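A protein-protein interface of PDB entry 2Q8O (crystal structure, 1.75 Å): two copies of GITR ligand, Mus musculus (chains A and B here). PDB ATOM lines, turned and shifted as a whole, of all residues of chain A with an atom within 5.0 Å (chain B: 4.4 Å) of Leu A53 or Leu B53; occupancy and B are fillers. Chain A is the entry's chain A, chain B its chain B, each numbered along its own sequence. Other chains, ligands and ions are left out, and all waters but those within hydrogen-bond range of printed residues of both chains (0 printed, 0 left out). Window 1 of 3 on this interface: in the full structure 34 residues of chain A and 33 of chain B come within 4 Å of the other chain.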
ATOM      1  N   THR A  51     -14.971   0.501  13.674  1.00  0.00           N
ATOM      2  CA  THR A  51     -15.570   1.508  14.520  1.00  0.00           C
ATOM      3  C   THR A  51     -15.674   2.794  13.692  1.00  0.00           C
ATOM      4  O   THR A  51     -14.671   3.271  13.139  1.00  0.00           O
ATOM      5  CB  THR A  51     -14.692   1.755  15.741  1.00  0.00           C
ATOM      6  OG1 THR A  51     -14.441   0.499  16.411  1.00  0.00           O
ATOM      7  CG2 THR A  51     -15.392   2.722  16.681  1.00  0.00           C
ATOM      8  N   TYR A  52     -16.895   3.310  13.587  1.00  0.00           N
ATOM      9  CA  TYR A  52     -17.181   4.516  12.811  1.00  0.00           C
ATOM     10  C   TYR A  52     -17.697   5.648  13.654  1.00  0.00           C
ATOM     11  O   TYR A  52     -18.415   5.428  14.623  1.00  0.00           O
ATOM     12  CB  TYR A  52     -18.177   4.245  11.688  1.00  0.00           C
ATOM     13  CG  TYR A  52     -17.600   3.392  10.577  1.00  0.00           C
ATOM     14  CD1 TYR A  52     -17.536   2.007  10.705  1.00  0.00           C
ATOM     15  CD2 TYR A  52     -17.145   3.982   9.394  1.00  0.00           C
ATOM     16  CE1 TYR A  52     -17.010   1.198   9.670  1.00  0.00           C
ATOM     17  CE2 TYR A  52     -16.622   3.193   8.362  1.00  0.00           C
ATOM     18  CZ  TYR A  52     -16.562   1.812   8.508  1.00  0.00           C
ATOM     19  OH  TYR A  52     -16.030   1.090   7.447  1.00  0.00           O
ATOM     20  N   LEU A  53     -17.383   6.870  13.233  1.00  0.00           N
ATOM     21  CA  LEU A  53     -18.030   8.041  13.780  1.00  0.00           C
ATOM     22  C   LEU A  53     -19.024   8.518  12.720  1.00  0.00           C
ATOM     23  O   LEU A  53     -18.615   8.908  11.619  1.00  0.00           O
ATOM     24  CB  LEU A  53     -16.971   9.100  14.100  1.00  0.00           C
ATOM     25  CG  LEU A  53     -17.455  10.468  14.542  1.00  0.00           C
ATOM     26  CD1 LEU A  53     -18.424  10.360  15.771  1.00  0.00           C
ATOM     27  CD2 LEU A  53     -16.183  11.269  14.892  1.00  0.00           C
ATOM     28  N   ILE A  54     -20.309   8.412  13.041  1.00  0.00           N
ATOM     29  CA  ILE A  54     -21.380   8.967  12.206  1.00  0.00           C
ATOM     30  C   ILE A  54     -21.602  10.383  12.703  1.00  0.00           C
ATOM     31  O   ILE A  54     -21.596  10.630  13.927  1.00  0.00           O
ATOM     32  CB  ILE A  54     -22.708   8.157  12.344  1.00  0.00           C
ATOM     33  CG1 ILE A  54     -22.489   6.686  11.961  1.00  0.00           C
ATOM     34  CG2 ILE A  54     -23.807   8.765  11.484  1.00  0.00           C
ATOM     35  CD1 ILE A  54     -23.732   5.729  12.254  1.00  0.00           C
ATOM     36  N   TYR A  55     -21.733  11.331  11.775  1.00  0.00           N
ATOM     37  CA  TYR A  55     -21.840  12.734  12.181  1.00  0.00           C
ATOM     38  C   TYR A  55     -22.755  13.496  11.231  1.00  0.00           C
ATOM     39  O   TYR A  55     -23.176  12.969  10.194  1.00  0.00           O
ATOM     40  CB  TYR A  55     -20.425  13.371  12.209  1.00  0.00           C
ATOM     41  CG  TYR A  55     -19.848  13.537  10.821  1.00  0.00           C
ATOM     42  CD1 TYR A  55     -20.055  14.728  10.111  1.00  0.00           C
ATOM     43  CD2 TYR A  55     -19.154  12.492  10.186  1.00  0.00           C
ATOM     44  CE1 TYR A  55     -19.560  14.887   8.801  1.00  0.00           C
ATOM     45  CE2 TYR A  55     -18.668  12.643   8.863  1.00  0.00           C
ATOM     46  CZ  TYR A  55     -18.891  13.828   8.189  1.00  0.00           C
ATOM     47  OH  TYR A  55     -18.401  13.957   6.893  1.00  0.00           O
ATOM     48  N   GLY A  97     -22.531   9.791  16.443  1.00  0.00           N
ATOM     49  CA  GLY A  97     -21.784   9.185  17.558  1.00  0.00           C
ATOM     50  C   GLY A  97     -20.920   8.033  17.055  1.00  0.00           C
ATOM     51  O   GLY A  97     -20.861   7.779  15.846  1.00  0.00           O
ATOM     52  N   VAL A  98     -20.240   7.370  17.993  1.00  0.00           N
ATOM     53  CA  VAL A  98     -19.343   6.252  17.705  1.00  0.00           C
ATOM     54  C   VAL A  98     -20.161   4.976  17.694  1.00  0.00           C
ATOM     55  O   VAL A  98     -20.857   4.655  18.681  1.00  0.00           O
ATOM     56  CB  VAL A  98     -18.249   6.143  18.786  1.00  0.00           C
ATOM     57  CG1 VAL A  98     -17.337   4.959  18.505  1.00  0.00           C
ATOM     58  CG2 VAL A  98     -17.402   7.403  18.784  1.00  0.00           C
ATOM     59  N   GLY A 125     -22.495  12.249   7.411  1.00  0.00           N
ATOM     60  CA  GLY A 125     -21.481  11.389   6.830  1.00  0.00           C
ATOM     61  C   GLY A 125     -20.925  10.429   7.840  1.00  0.00           C
ATOM     62  O   GLY A 125     -21.468  10.272   8.946  1.00  0.00           O
ATOM     63  N   ILE A 126     -19.841   9.760   7.452  1.00  0.00           N
ATOM     64  CA  ILE A 126     -19.149   8.854   8.366  1.00  0.00           C
ATOM     65  C   ILE A 126     -17.636   8.970   8.242  1.00  0.00           C
ATOM     66  O   ILE A 126     -17.111   9.475   7.240  1.00  0.00           O
ATOM     67  CB  ILE A 126     -19.541   7.350   8.185  1.00  0.00           C
ATOM     68  CG1 ILE A 126     -19.199   6.828   6.778  1.00  0.00           C
ATOM     69  CG2 ILE A 126     -21.005   7.103   8.533  1.00  0.00           C
ATOM     70  CD1 ILE A 126     -19.390   5.314   6.634  1.00  0.00           C
ATOM     71  N   ILE A 127     -16.960   8.496   9.284  1.00  0.00           N
ATOM     72  CA  ILE A 127     -15.505   8.380   9.324  1.00  0.00           C
ATOM     73  C   ILE A 127     -15.185   6.995   9.847  1.00  0.00           C
ATOM     74  O   ILE A 127     -15.774   6.555  10.848  1.00  0.00           O
ATOM     75  CB  ILE A 127     -14.876   9.383  10.315  1.00  0.00           C
ATOM     76  CG1 ILE A 127     -15.212  10.809   9.903  1.00  0.00           C
ATOM     77  CG2 ILE A 127     -13.351   9.165  10.425  1.00  0.00           C
ATOM     78  CD1 ILE A 127     -14.985  11.836  11.029  1.00  0.00           C
ATOM     79  N   MET A 129     -12.888   5.193  12.005  1.00  0.00           N
ATOM     80  CA  MET A 129     -12.002   5.726  13.037  1.00  0.00           C
ATOM     81  C   MET A 129     -10.650   5.005  13.093  1.00  0.00           C
ATOM     82  O   MET A 129     -10.575   3.813  12.855  1.00  0.00           O
ATOM     83  CB  MET A 129     -12.688   5.662  14.414  1.00  0.00           C
ATOM     84  CG  MET A 129     -13.762   6.733  14.567  1.00  0.00           C
ATOM     85  SD  MET A 129     -14.815   6.407  16.002  1.00  0.00           S
ATOM     86  CE  MET A 129     -13.619   6.024  17.287  1.00  0.00           C
ATOM     87  N   MET B  16      -6.859  11.742  16.652  1.00  0.00           N
ATOM     88  CA  MET B  16      -8.191  11.671  17.265  1.00  0.00           C
ATOM     89  C   MET B  16      -8.072  11.376  18.751  1.00  0.00           C
ATOM     90  O   MET B  16      -7.236  10.562  19.165  1.00  0.00           O
ATOM     91  CB  MET B  16      -9.046  10.565  16.626  1.00  0.00           C
ATOM     92  CG  MET B  16     -10.435  10.442  17.253  1.00  0.00           C
ATOM     93  SD  MET B  16     -11.423   9.211  16.387  1.00  0.00           S
ATOM     94  CE  MET B  16     -13.061   9.599  17.026  1.00  0.00           C
ATOM     95  N   TYR B  52     -11.740  20.329  11.862  1.00  0.00           N
ATOM     96  CA  TYR B  52     -11.997  19.298  12.880  1.00  0.00           C
ATOM     97  C   TYR B  52     -13.447  18.889  12.943  1.00  0.00           C
ATOM     98  O   TYR B  52     -14.333  19.692  12.677  1.00  0.00           O
ATOM     99  CB  TYR B  52     -11.621  19.821  14.282  1.00  0.00           C
ATOM    100  CG  TYR B  52     -10.142  19.897  14.468  1.00  0.00           C
ATOM    101  CD1 TYR B  52      -9.433  21.019  14.020  1.00  0.00           C
ATOM    102  CD2 TYR B  52      -9.446  18.864  15.095  1.00  0.00           C
ATOM    103  CE1 TYR B  52      -8.057  21.120  14.169  1.00  0.00           C
ATOM    104  CE2 TYR B  52      -8.065  18.950  15.270  1.00  0.00           C
ATOM    105  CZ  TYR B  52      -7.382  20.074  14.787  1.00  0.00           C
ATOM    106  OH  TYR B  52      -6.036  20.147  14.955  1.00  0.00           O
ATOM    107  N   LEU B  53     -13.674  17.630  13.290  1.00  0.00           N
ATOM    108  CA  LEU B  53     -14.974  17.198  13.738  1.00  0.00           C
ATOM    109  C   LEU B  53     -14.892  17.258  15.251  1.00  0.00           C
ATOM    110  O   LEU B  53     -13.982  16.667  15.853  1.00  0.00           O
ATOM    111  CB  LEU B  53     -15.235  15.757  13.295  1.00  0.00           C
ATOM    112  CG  LEU B  53     -16.598  15.435  12.691  1.00  0.00           C
ATOM    113  CD1 LEU B  53     -16.692  13.927  12.401  1.00  0.00           C
ATOM    114  CD2 LEU B  53     -17.785  15.944  13.553  1.00  0.00           C
ATOM    115  N   ILE B  54     -15.811  18.000  15.861  1.00  0.00           N
ATOM    116  CA  ILE B  54     -15.993  17.945  17.302  1.00  0.00           C
ATOM    117  C   ILE B  54     -17.206  17.031  17.464  1.00  0.00           C
ATOM    118  O   ILE B  54     -18.211  17.176  16.754  1.00  0.00           O
ATOM    119  CB  ILE B  54     -16.295  19.335  17.905  1.00  0.00           C
ATOM    120  CG1 ILE B  54     -15.130  20.300  17.666  1.00  0.00           C
ATOM    121  CG2 ILE B  54     -16.678  19.186  19.393  1.00  0.00           C
ATOM    122  CD1 ILE B  54     -15.424  21.775  18.112  1.00  0.00           C
ATOM    123  N   TYR B  55     -17.109  16.046  18.349  1.00  0.00           N
ATOM    124  CA  TYR B  55     -18.168  15.041  18.444  1.00  0.00           C
ATOM    125  C   TYR B  55     -18.393  14.630  19.914  1.00  0.00           C
ATOM    126  O   TYR B  55     -17.623  15.011  20.816  1.00  0.00           O
ATOM    127  CB  TYR B  55     -17.837  13.810  17.560  1.00  0.00           C
ATOM    128  CG  TYR B  55     -16.689  13.001  18.166  1.00  0.00           C
ATOM    129  CD1 TYR B  55     -16.954  11.900  19.007  1.00  0.00           C
ATOM    130  CD2 TYR B  55     -15.360  13.370  17.935  1.00  0.00           C
ATOM    131  CE1 TYR B  55     -15.920  11.198  19.628  1.00  0.00           C
ATOM    132  CE2 TYR B  55     -14.288  12.673  18.574  1.00  0.00           C
ATOM    133  CZ  TYR B  55     -14.598  11.579  19.402  1.00  0.00           C
ATOM    134  OH  TYR B  55     -13.590  10.898  20.038  1.00  0.00           O
ATOM    135  N   GLY B  97     -19.992  18.948  15.348  1.00  0.00           N
ATOM    136  CA  GLY B  97     -20.094  19.177  13.909  1.00  0.00           C
ATOM    137  C   GLY B  97     -18.713  19.549  13.407  1.00  0.00           C
ATOM    138  O   GLY B  97     -17.737  19.440  14.159  1.00  0.00           O
ATOM    139  N   VAL B  98     -18.650  19.946  12.134  1.00  0.00           N
ATOM    140  CA  VAL B  98     -17.399  20.288  11.484  1.00  0.00           C
ATOM    141  C   VAL B  98     -17.114  21.776  11.733  1.00  0.00           C
ATOM    142  O   VAL B  98     -17.942  22.652  11.422  1.00  0.00           O
ATOM    143  CB  VAL B  98     -17.463  20.041   9.968  1.00  0.00           C
ATOM    144  CG1 VAL B  98     -16.180  20.486   9.312  1.00  0.00           C
ATOM    145  CG2 VAL B  98     -17.742  18.556   9.664  1.00  0.00           C
ATOM    146  N   GLY B 125     -15.023  14.449  22.056  1.00  0.00           N
ATOM    147  CA  GLY B 125     -13.663  14.636  21.603  1.00  0.00           C
ATOM    148  C   GLY B 125     -13.577  15.342  20.281  1.00  0.00           C
ATOM    149  O   GLY B 125     -14.512  16.012  19.873  1.00  0.00           O
ATOM    150  N   ILE B 126     -12.425  15.212  19.626  1.00  0.00           N
ATOM    151  CA  ILE B 126     -12.225  15.757  18.287  1.00  0.00           C
ATOM    152  C   ILE B 126     -11.425  14.811  17.408  1.00  0.00           C
ATOM    153  O   ILE B 126     -10.725  13.901  17.891  1.00  0.00           O
ATOM    154  CB  ILE B 126     -11.526  17.149  18.266  1.00  0.00           C
ATOM    155  CG1 ILE B 126     -10.165  17.083  18.972  1.00  0.00           C
ATOM    156  CG2 ILE B 126     -12.421  18.252  18.852  1.00  0.00           C
ATOM    157  CD1 ILE B 126      -9.284  18.237  18.696  1.00  0.00           C
ATOM    158  N   ILE B 127     -11.542  15.037  16.108  1.00  0.00           N
ATOM    159  CA  ILE B 127     -10.691  14.365  15.130  1.00  0.00           C
ATOM    160  C   ILE B 127     -10.289  15.379  14.074  1.00  0.00           C
ATOM    161  O   ILE B 127     -11.122  16.142  13.577  1.00  0.00           O
ATOM    162  CB  ILE B 127     -11.348  13.118  14.482  1.00  0.00           C
ATOM    163  CG1 ILE B 127     -10.430  12.526  13.393  1.00  0.00           C
ATOM    164  CG2 ILE B 127     -12.726  13.436  13.926  1.00  0.00           C
ATOM    165  CD1 ILE B 127     -10.844  11.067  13.000  1.00  0.00           C
ATOM    166  N   MET B 129      -9.694  16.351  10.566  1.00  0.00           N
ATOM    167  CA  MET B 129     -10.256  15.763   9.347  1.00  0.00           C
ATOM    168  C   MET B 129      -9.358  15.932   8.121  1.00  0.00           C
ATOM    169  O   MET B 129      -8.879  17.050   7.869  1.00  0.00           O
ATOM    170  CB  MET B 129     -11.658  16.319   9.060  1.00  0.00           C
ATOM    171  CG  MET B 129     -12.749  15.656   9.889  1.00  0.00           C
ATOM    172  SD  MET B 129     -14.417  16.024   9.329  1.00  0.00           S
ATOM    173  CE  MET B 129     -14.555  17.674   9.960  1.00  0.00           C
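Among the printed residues, pairs that only touch across the chains: Leu A53 with Leu B53, Leu A53 with Tyr B55, Tyr A55 with Leu B53, Ile A127 with Leu B53 and Met A129 with Met B16.
The backbone NH (N) of Ile B127 sits at hydrogen-bond distance from the backbone carbonyl oxygen (O) of Leu B53 (2.9 Å). The backbone carbonyl oxygen (O) of Thr A51 is in hydrogen-bond range of the backbone NH (N) of Met A129 (2.9 Å). The backbone NH (N) of Gly B125 is in hydrogen-bond range of the backbone carbonyl oxygen (O) of Tyr B55. The backbone carbonyl oxygen (O) of Tyr A55 is in hydrogen-bond range of the backbone NH (N) of Gly A125, 3.0 Å away. N of Ile A127 lies within hydrogen-bond range of O of Leu A53, at 2.9 Å.
Printed residues of chain B within 4 Å of Leu A53: Leu B53 (3.7 Å) and Tyr B55 (3.7 Å). Of the printed residues of chain B, Tyr A55 touches Leu B53 (3.6 Å). Of the printed residues of chain B, Ile A127 touches Leu B53 (3.0 Å). Printed residues of chain A within 4 Å of Met B16: Met A129. Printed residues of chain A within 4 Å of Leu B53: Leu A53, Tyr A55 and Ile A127. Of the printed residues of chain A, Tyr B55 touches Leu A53 (3.7 Å).
Leu B53 touches its own counterpart, Leu A53. Leu A53 touches Tyr B55, and with the chains exchanged Tyr A55 touches Leu B53. Ile A127 touches Leu B53, but with the chains exchanged Leu A53 does not touch Ile B127 (4.2 Å). Positions printed for both chains: 52, 53, 54, 55, 97, 98, 125, 126, 127 and 129.
Hydrophobic or aromatic side chains of chain B within 4 Å of the printed part of chain A: Met B16, Leu B53 and Tyr B55. Among the printed residues, 5 pairs touch across the chains. Among the printed residues, no Asp or Glu carboxylate lies within 4 Å of a Lys or Arg side-chain nitrogen of the other chain.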
